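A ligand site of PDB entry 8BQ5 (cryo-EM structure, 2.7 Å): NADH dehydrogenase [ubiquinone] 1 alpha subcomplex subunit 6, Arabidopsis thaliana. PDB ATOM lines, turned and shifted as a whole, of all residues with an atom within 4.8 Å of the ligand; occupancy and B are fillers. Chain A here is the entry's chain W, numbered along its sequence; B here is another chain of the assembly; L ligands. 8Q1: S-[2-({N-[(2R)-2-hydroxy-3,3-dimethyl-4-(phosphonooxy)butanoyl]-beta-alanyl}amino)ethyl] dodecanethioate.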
ATOM      1  N   ARG A  23       0.329  -2.794  14.240  1.00  0.00           N
ATOM      2  CA  ARG A  23       1.278  -3.458  15.176  1.00  0.00           C
ATOM      3  C   ARG A  23       0.762  -3.296  16.599  1.00  0.00           C
ATOM      4  O   ARG A  23       0.966  -4.216  17.415  1.00  0.00           O
ATOM      5  CB  ARG A  23       2.691  -2.883  14.977  1.00  0.00           C
ATOM      6  CG  ARG A  23       3.785  -3.594  15.754  1.00  0.00           C
ATOM      7  CD  ARG A  23       5.115  -2.865  15.744  1.00  0.00           C
ATOM      8  NE  ARG A  23       5.028  -1.436  15.475  1.00  0.00           N
ATOM      9  CZ  ARG A  23       5.446  -0.846  14.363  1.00  0.00           C
ATOM     10  NH1 ARG A  23       5.972  -1.559  13.386  1.00  0.00           N
ATOM     11  NH2 ARG A  23       5.313   0.457  14.225  1.00  0.00           N
ATOM     12  N   VAL A  26      -1.500  -6.000  17.028  1.00  0.00           N
ATOM     13  CA  VAL A  26      -0.744  -7.285  17.134  1.00  0.00           C
ATOM     14  C   VAL A  26      -0.384  -7.538  18.594  1.00  0.00           C
ATOM     15  O   VAL A  26      -0.510  -8.687  19.040  1.00  0.00           O
ATOM     16  CB  VAL A  26       0.512  -7.290  16.228  1.00  0.00           C
ATOM     17  CG1 VAL A  26       1.436  -8.460  16.499  1.00  0.00           C
ATOM     18  CG2 VAL A  26       0.157  -7.231  14.755  1.00  0.00           C
ATOM     19  N   PHE A  27       0.027  -6.493  19.314  1.00  0.00           N
ATOM     20  CA  PHE A  27       0.467  -6.693  20.714  1.00  0.00           C
ATOM     21  C   PHE A  27      -0.758  -7.021  21.586  1.00  0.00           C
ATOM     22  O   PHE A  27      -0.619  -7.923  22.398  1.00  0.00           O
ATOM     23  CB  PHE A  27       1.316  -5.513  21.196  1.00  0.00           C
ATOM     24  CG  PHE A  27       2.636  -5.387  20.482  1.00  0.00           C
ATOM     25  CD1 PHE A  27       3.281  -6.510  19.988  1.00  0.00           C
ATOM     26  CD2 PHE A  27       3.234  -4.151  20.301  1.00  0.00           C
ATOM     27  CE1 PHE A  27       4.488  -6.403  19.309  1.00  0.00           C
ATOM     28  CE2 PHE A  27       4.451  -4.049  19.641  1.00  0.00           C
ATOM     29  CZ  PHE A  27       5.079  -5.171  19.150  1.00  0.00           C
ATOM     30  N   PHE A  29      -3.402  -8.629  20.689  1.00  0.00           N
ATOM     31  CA  PHE A  29      -3.698 -10.029  20.440  1.00  0.00           C
ATOM     32  C   PHE A  29      -2.691 -10.944  21.131  1.00  0.00           C
ATOM     33  O   PHE A  29      -3.071 -11.972  21.701  1.00  0.00           O
ATOM     34  CB  PHE A  29      -3.718 -10.319  18.943  1.00  0.00           C
ATOM     35  CG  PHE A  29      -3.632 -11.783  18.619  1.00  0.00           C
ATOM     36  CD1 PHE A  29      -4.719 -12.600  18.798  1.00  0.00           C
ATOM     37  CD2 PHE A  29      -2.448 -12.335  18.160  1.00  0.00           C
ATOM     38  CE1 PHE A  29      -4.660 -13.944  18.527  1.00  0.00           C
ATOM     39  CE2 PHE A  29      -2.372 -13.680  17.885  1.00  0.00           C
ATOM     40  CZ  PHE A  29      -3.482 -14.481  18.059  1.00  0.00           C
ATOM     41  N   ALA A  33      -3.996 -13.589  23.777  1.00  0.00           N
ATOM     42  CA  ALA A  33      -3.815 -15.012  23.495  1.00  0.00           C
ATOM     43  C   ALA A  33      -2.928 -15.676  24.529  1.00  0.00           C
ATOM     44  O   ALA A  33      -3.190 -16.806  24.944  1.00  0.00           O
ATOM     45  CB  ALA A  33      -3.241 -15.212  22.084  1.00  0.00           C
ATOM     46  N   ILE A  40      -5.842 -22.715  29.168  1.00  0.00           N
ATOM     47  CA  ILE A  40      -5.598 -23.814  28.235  1.00  0.00           C
ATOM     48  C   ILE A  40      -4.927 -24.978  28.949  1.00  0.00           C
ATOM     49  O   ILE A  40      -5.188 -26.144  28.637  1.00  0.00           O
ATOM     50  CB  ILE A  40      -4.781 -23.307  27.029  1.00  0.00           C
ATOM     51  CG1 ILE A  40      -5.676 -22.513  26.073  1.00  0.00           C
ATOM     52  CG2 ILE A  40      -4.127 -24.464  26.289  1.00  0.00           C
ATOM     53  CD1 ILE A  40      -4.913 -21.611  25.131  1.00  0.00           C
ATOM     54  N   ILE A  59       3.374 -19.125  20.310  1.00  0.00           N
ATOM     55  CA  ILE A  59       2.571 -17.976  19.786  1.00  0.00           C
ATOM     56  C   ILE A  59       3.522 -16.913  19.241  1.00  0.00           C
ATOM     57  O   ILE A  59       3.289 -16.424  18.120  1.00  0.00           O
ATOM     58  CB  ILE A  59       1.620 -17.407  20.852  1.00  0.00           C
ATOM     59  CG1 ILE A  59       0.784 -18.505  21.526  1.00  0.00           C
ATOM     60  CG2 ILE A  59       0.735 -16.323  20.273  1.00  0.00           C
ATOM     61  CD1 ILE A  59       0.247 -18.108  22.873  1.00  0.00           C
ATOM     62  N   GLN A  62       4.856 -17.790  15.863  1.00  0.00           N
ATOM     63  CA  GLN A  62       3.889 -17.582  14.790  1.00  0.00           C
ATOM     64  C   GLN A  62       3.830 -16.112  14.385  1.00  0.00           C
ATOM     65  O   GLN A  62       3.742 -15.787  13.201  1.00  0.00           O
ATOM     66  CB  GLN A  62       2.515 -18.077  15.225  1.00  0.00           C
ATOM     67  CG  GLN A  62       1.764 -18.888  14.185  1.00  0.00           C
ATOM     68  CD  GLN A  62       2.351 -20.271  13.960  1.00  0.00           C
ATOM     69  OE1 GLN A  62       3.406 -20.614  14.497  1.00  0.00           O
ATOM     70  NE2 GLN A  62       1.662 -21.075  13.149  1.00  0.00           N
ATOM     71  N   ILE A  63       3.876 -15.210  15.364  1.00  0.00           N
ATOM     72  CA  ILE A  63       3.862 -13.781  15.074  1.00  0.00           C
ATOM     73  C   ILE A  63       5.134 -13.377  14.339  1.00  0.00           C
ATOM     74  O   ILE A  63       5.094 -12.587  13.394  1.00  0.00           O
ATOM     75  CB  ILE A  63       3.669 -12.980  16.380  1.00  0.00           C
ATOM     76  CG1 ILE A  63       2.261 -13.176  16.928  1.00  0.00           C
ATOM     77  CG2 ILE A  63       3.962 -11.504  16.152  1.00  0.00           C
ATOM     78  CD1 ILE A  63       1.984 -12.376  18.178  1.00  0.00           C
ATOM     79  N   ASN A  66       5.604 -13.967  10.530  1.00  0.00           N
ATOM     80  CA  ASN A  66       4.897 -13.039   9.658  1.00  0.00           C
ATOM     81  C   ASN A  66       5.393 -11.612   9.805  1.00  0.00           C
ATOM     82  O   ASN A  66       4.710 -10.677   9.397  1.00  0.00           O
ATOM     83  CB  ASN A  66       3.391 -13.103   9.921  1.00  0.00           C
ATOM     84  CG  ASN A  66       2.771 -14.388   9.443  1.00  0.00           C
ATOM     85  OD1 ASN A  66       2.167 -15.132  10.217  1.00  0.00           O
ATOM     86  ND2 ASN A  66       2.902 -14.672   8.152  1.00  0.00           N
ATOM     87  N   ALA A  67       6.592 -11.424  10.380  1.00  0.00           N
ATOM     88  CA  ALA A  67       7.101 -10.080  10.621  1.00  0.00           C
ATOM     89  C   ALA A  67       7.411  -9.326   9.336  1.00  0.00           C
ATOM     90  O   ALA A  67       7.585  -8.098   9.385  1.00  0.00           O
ATOM     91  CB  ALA A  67       8.369 -10.152  11.474  1.00  0.00           C
ATOM     92  N   HIS A  68       7.477 -10.009   8.194  1.00  0.00           N
ATOM     93  CA  HIS A  68       7.785  -9.389   6.918  1.00  0.00           C
ATOM     94  C   HIS A  68       6.572  -8.768   6.230  1.00  0.00           C
ATOM     95  O   HIS A  68       6.743  -8.098   5.208  1.00  0.00           O
ATOM     96  CB  HIS A  68       8.415 -10.416   5.990  1.00  0.00           C
ATOM     97  CG  HIS A  68       7.714 -11.742   6.005  1.00  0.00           C
ATOM     98  ND1 HIS A  68       6.400 -11.884   5.598  1.00  0.00           N
ATOM     99  CD2 HIS A  68       8.118 -12.968   6.407  1.00  0.00           C
ATOM    100  CE1 HIS A  68       6.037 -13.152   5.729  1.00  0.00           C
ATOM    101  NE2 HIS A  68       7.067 -13.827   6.220  1.00  0.00           N
ATOM    102  N   ILE A  69       5.364  -8.993   6.753  1.00  0.00           N
ATOM    103  CA  ILE A  69       4.169  -8.445   6.123  1.00  0.00           C
ATOM    104  C   ILE A  69       4.145  -6.928   6.302  1.00  0.00           C
ATOM    105  O   ILE A  69       4.382  -6.423   7.402  1.00  0.00           O
ATOM    106  CB  ILE A  69       2.904  -9.088   6.698  1.00  0.00           C
ATOM    107  CG1 ILE A  69       3.019 -10.618   6.702  1.00  0.00           C
ATOM    108  CG2 ILE A  69       1.664  -8.623   5.943  1.00  0.00           C
ATOM    109  CD1 ILE A  69       2.677 -11.263   5.383  1.00  0.00           C
ATOM    110  N   ILE A  75      -2.451  -7.788   7.951  1.00  0.00           N
ATOM    111  CA  ILE A  75      -2.225  -7.951   9.390  1.00  0.00           C
ATOM    112  C   ILE A  75      -3.557  -8.009  10.130  1.00  0.00           C
ATOM    113  O   ILE A  75      -3.735  -8.834  11.035  1.00  0.00           O
ATOM    114  CB  ILE A  75      -1.326  -6.825   9.926  1.00  0.00           C
ATOM    115  CG1 ILE A  75       0.084  -6.953   9.346  1.00  0.00           C
ATOM    116  CG2 ILE A  75      -1.276  -6.856  11.434  1.00  0.00           C
ATOM    117  CD1 ILE A  75       1.022  -5.846   9.794  1.00  0.00           C
ATOM    118  N   LEU A  78      -5.049 -11.400   9.685  1.00  0.00           N
ATOM    119  CA  LEU A  78      -4.328 -12.420  10.441  1.00  0.00           C
ATOM    120  C   LEU A  78      -4.694 -12.381  11.914  1.00  0.00           C
ATOM    121  O   LEU A  78      -4.828 -13.429  12.557  1.00  0.00           O
ATOM    122  CB  LEU A  78      -2.813 -12.240  10.253  1.00  0.00           C
ATOM    123  CG  LEU A  78      -2.211 -12.641   8.910  1.00  0.00           C
ATOM    124  CD1 LEU A  78      -0.751 -12.204   8.844  1.00  0.00           C
ATOM    125  CD2 LEU A  78      -2.315 -14.135   8.677  1.00  0.00           C
ATOM    126  N   ILE A  79      -4.838 -11.186  12.478  1.00  0.00           N
ATOM    127  CA  ILE A  79      -5.237 -11.061  13.879  1.00  0.00           C
ATOM    128  C   ILE A  79      -6.645 -11.587  14.084  1.00  0.00           C
ATOM    129  O   ILE A  79      -6.931 -12.275  15.072  1.00  0.00           O
ATOM    130  CB  ILE A  79      -5.107  -9.600  14.352  1.00  0.00           C
ATOM    131  CG1 ILE A  79      -3.669  -9.103  14.160  1.00  0.00           C
ATOM    132  CG2 ILE A  79      -5.536  -9.468  15.801  1.00  0.00           C
ATOM    133  CD1 ILE A  79      -2.733  -9.549  15.262  1.00  0.00           C
ATOM    134  N   GLY A  82      -6.537 -15.117  14.101  1.00  0.00           N
ATOM    135  CA  GLY A  82      -5.892 -15.540  15.330  1.00  0.00           C
ATOM    136  C   GLY A  82      -6.833 -15.543  16.515  1.00  0.00           C
ATOM    137  O   GLY A  82      -6.812 -16.467  17.339  1.00  0.00           O
ATOM    138  N   GLU A  85      -9.104 -18.571  16.061  1.00  0.00           N
ATOM    139  CA  GLU A  85      -8.379 -19.782  16.436  1.00  0.00           C
ATOM    140  C   GLU A  85      -8.266 -19.903  17.939  1.00  0.00           C
ATOM    141  O   GLU A  85      -8.449 -20.985  18.504  1.00  0.00           O
ATOM    142  CB  GLU A  85      -6.983 -19.781  15.792  1.00  0.00           C
ATOM    143  CG  GLU A  85      -6.929 -20.398  14.407  1.00  0.00           C
ATOM    144  CD  GLU A  85      -5.779 -19.855  13.576  1.00  0.00           C
ATOM    145  OE1 GLU A  85      -6.003 -19.499  12.407  1.00  0.00           O
ATOM    146  OE2 GLU A  85      -4.649 -19.774  14.115  1.00  0.00           O
ATOM    147  N   LEU A  86      -7.961 -18.786  18.608  1.00  0.00           N
ATOM    148  CA  LEU A  86      -7.866 -18.789  20.066  1.00  0.00           C
ATOM    149  C   LEU A  86      -9.203 -19.120  20.720  1.00  0.00           C
ATOM    150  O   LEU A  86      -9.253 -19.920  21.661  1.00  0.00           O
ATOM    151  CB  LEU A  86      -7.394 -17.418  20.539  1.00  0.00           C
ATOM    152  CG  LEU A  86      -7.337 -17.249  22.060  1.00  0.00           C
ATOM    153  CD1 LEU A  86      -6.397 -18.259  22.695  1.00  0.00           C
ATOM    154  CD2 LEU A  86      -6.984 -15.819  22.424  1.00  0.00           C
ATOM    155  N   ILE A  89     -10.119 -22.748  20.559  1.00  0.00           N
ATOM    156  CA  ILE A  89      -9.267 -23.556  21.430  1.00  0.00           C
ATOM    157  C   ILE A  89      -9.776 -23.499  22.866  1.00  0.00           C
ATOM    158  O   ILE A  89      -9.782 -24.512  23.574  1.00  0.00           O
ATOM    159  CB  ILE A  89      -7.797 -23.102  21.322  1.00  0.00           C
ATOM    160  CG1 ILE A  89      -7.116 -23.829  20.160  1.00  0.00           C
ATOM    161  CG2 ILE A  89      -7.044 -23.338  22.618  1.00  0.00           C
ATOM    162  CD1 ILE A  89      -5.730 -23.313  19.860  1.00  0.00           C
ATOM    163  N   TYR A 103      -1.031 -26.872  16.430  1.00  0.00           N
ATOM    164  CA  TYR A 103       0.317 -26.875  16.969  1.00  0.00           C
ATOM    165  C   TYR A 103       0.595 -28.150  17.765  1.00  0.00           C
ATOM    166  O   TYR A 103      -0.184 -28.538  18.640  1.00  0.00           O
ATOM    167  CB  TYR A 103       0.551 -25.646  17.845  1.00  0.00           C
ATOM    168  CG  TYR A 103       0.023 -24.382  17.207  1.00  0.00           C
ATOM    169  CD1 TYR A 103      -1.016 -23.662  17.782  1.00  0.00           C
ATOM    170  CD2 TYR A 103       0.533 -23.929  15.999  1.00  0.00           C
ATOM    171  CE1 TYR A 103      -1.508 -22.523  17.198  1.00  0.00           C
ATOM    172  CE2 TYR A 103       0.044 -22.791  15.398  1.00  0.00           C
ATOM    173  CZ  TYR A 103      -0.967 -22.085  16.001  1.00  0.00           C
ATOM    174  OH  TYR A 103      -1.460 -20.939  15.405  1.00  0.00           O
ATOM    175  N   ASP B  82      13.716  -6.473  21.085  1.00  0.00           N
ATOM    176  CA  ASP B  82      12.836  -5.586  20.272  1.00  0.00           C
ATOM    177  C   ASP B  82      11.460  -5.488  20.919  1.00  0.00           C
ATOM    178  O   ASP B  82      11.320  -5.954  22.062  1.00  0.00           O
ATOM    179  CB  ASP B  82      12.785  -6.021  18.800  1.00  0.00           C
ATOM    180  CG  ASP B  82      12.404  -7.476  18.588  1.00  0.00           C
ATOM    181  OD1 ASP B  82      12.070  -8.162  19.569  1.00  0.00           O
ATOM    182  OD2 ASP B  82      12.448  -7.912  17.415  1.00  0.00           O
ATOM    183  N   SER B  83      10.466  -4.917  20.217  1.00  0.00           N
ATOM    184  CA  SER B  83       9.152  -4.678  20.878  1.00  0.00           C
ATOM    185  C   SER B  83       8.451  -5.998  21.220  1.00  0.00           C
ATOM    186  O   SER B  83       7.917  -6.087  22.348  1.00  0.00           O
ATOM    187  CB  SER B  83       8.268  -3.729  20.110  1.00  0.00           C
ATOM    188  OG  SER B  83       7.836  -4.286  18.886  1.00  0.00           O
ATOM    189  N   LEU B  84       8.474  -6.981  20.318  1.00  0.00           N
ATOM    190  CA  LEU B  84       7.769  -8.267  20.574  1.00  0.00           C
ATOM    191  C   LEU B  84       8.487  -8.987  21.722  1.00  0.00           C
ATOM    192  O   LEU B  84       7.790  -9.560  22.576  1.00  0.00           O
ATOM    193  CB  LEU B  84       7.753  -9.096  19.292  1.00  0.00           C
ATOM    194  CG  LEU B  84       6.931 -10.381  19.364  1.00  0.00           C
ATOM    195  CD1 LEU B  84       5.505 -10.098  19.789  1.00  0.00           C
ATOM    196  CD2 LEU B  84       6.953 -11.111  18.034  1.00  0.00           C
HETATM  197  O4  8Q1 L   1       1.055 -13.553  12.633  1.00  0.00           O
HETATM  198  C16 8Q1 L   1      -2.922 -20.949  21.703  1.00  0.00           C
HETATM  199  O3  8Q1 L   1       9.466  -5.711  17.634  1.00  0.00           O
HETATM  200  C15 8Q1 L   1      -2.823 -20.447  20.275  1.00  0.00           C
HETATM  201  C14 8Q1 L   1      -4.017 -19.659  19.828  1.00  0.00           C
HETATM  202  C13 8Q1 L   1      -3.689 -18.442  19.007  1.00  0.00           C
HETATM  203  O2  8Q1 L   1      10.330  -5.222  15.306  1.00  0.00           O
HETATM  204  C12 8Q1 L   1      -3.085 -18.770  17.673  1.00  0.00           C
HETATM  205  C11 8Q1 L   1      -1.977 -17.839  17.243  1.00  0.00           C
HETATM  206  C10 8Q1 L   1      -2.102 -17.352  15.825  1.00  0.00           C
HETATM  207  C9  8Q1 L   1      -1.064 -16.352  15.409  1.00  0.00           C
HETATM  208  C8  8Q1 L   1      -1.066 -16.049  13.939  1.00  0.00           C
HETATM  209  C7  8Q1 L   1      -1.581 -14.661  13.593  1.00  0.00           C
HETATM  210  C6  8Q1 L   1      -0.757 -13.568  14.182  1.00  0.00           C
HETATM  211  C1  8Q1 L   1       0.192 -12.943  13.212  1.00  0.00           C
HETATM  212  C28 8Q1 L   1       7.297  -6.535  16.013  1.00  0.00           C
HETATM  213  C29 8Q1 L   1       7.442  -7.386  14.747  1.00  0.00           C
HETATM  214  C30 8Q1 L   1       8.642  -8.322  14.943  1.00  0.00           C
HETATM  215  C31 8Q1 L   1       6.189  -8.258  14.590  1.00  0.00           C
HETATM  216  C32 8Q1 L   1       7.646  -6.493  13.498  1.00  0.00           C
HETATM  217  C34 8Q1 L   1       6.372  -6.087  12.769  1.00  0.00           C
HETATM  218  C37 8Q1 L   1       4.953  -6.344  10.788  1.00  0.00           C
HETATM  219  C38 8Q1 L   1       4.133  -7.594  10.528  1.00  0.00           C
HETATM  220  C39 8Q1 L   1       3.474  -8.118  11.784  1.00  0.00           C
HETATM  221  C42 8Q1 L   1       2.441 -10.119  12.762  1.00  0.00           C
HETATM  222  C43 8Q1 L   1       1.330 -10.742  11.961  1.00  0.00           C
HETATM  223  N36 8Q1 L   1       6.137  -6.631  11.580  1.00  0.00           N
HETATM  224  N41 8Q1 L   1       3.409  -9.439  11.917  1.00  0.00           N
HETATM  225  O27 8Q1 L   1       7.861  -5.210  15.776  1.00  0.00           O
HETATM  226  O33 8Q1 L   1       8.556  -7.092  12.584  1.00  0.00           O
HETATM  227  O35 8Q1 L   1       5.628  -5.250  13.267  1.00  0.00           O
HETATM  228  O40 8Q1 L   1       3.013  -7.345  12.628  1.00  0.00           O
HETATM  229  P24 8Q1 L   1       9.323  -4.856  16.382  1.00  0.00           P
HETATM  230  S44 8Q1 L   1      -0.063 -11.212  13.011  1.00  0.00           S
HETATM  231  O1  8Q1 L   1       9.279  -3.376  16.674  1.00  0.00           O
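An oxygen (O4) of the ligand sits close to the side-chain amide oxygen (OD1) of Asn 66, 3.1 Å away.
The backbone carbonyl oxygen of Asn 66 sits at hydrogen-bond distance from a nitrogen (N41) of the ligand (3.1 Å).
OG of Ser 83 of chain B lies within hydrogen-bond range of O3 of the ligand (2.5 Å).
The backbone NH (N) of Leu 84 of chain B sits at hydrogen-bond distance from an oxygen (O3) of the ligand (3.1 Å).
The backbone NH (N) of Ser 83 of chain B is in hydrogen-bond range of an oxygen (O3) of the ligand (2.9 Å).
A nitrogen (N36) of the ligand is in hydrogen-bond range of the backbone carbonyl oxygen (O) of Ala 67, at 3.0 Å.
O of Gln 62 lies close to OD1 of Asn 66.
Merely in contact with the ligand: Ile 69 (3.3 Å), Arg 23 (3.5 Å), Asp 82 of chain B (3.5 Å), Tyr 103 (3.5 Å), Gln 62 (3.5 Å), Val 26 (3.6 Å), Leu 78 (3.6 Å), Ile 75 (3.6 Å), Ile 63 (3.7 Å), Phe 29 (3.8 Å), Ile 79 (3.9 Å), Glu 85 (3.9 Å) and Leu 86 (3.95 Å).
Hydrophobic or aromatic side chains within 4 Å of the ligand: Val 26, Phe 29, Ile 63, Ala 67, Ile 75, Ile 79, Leu 86 and Tyr 103.
Of the 24 residues printed, 17 come within 4 Å of the ligand.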
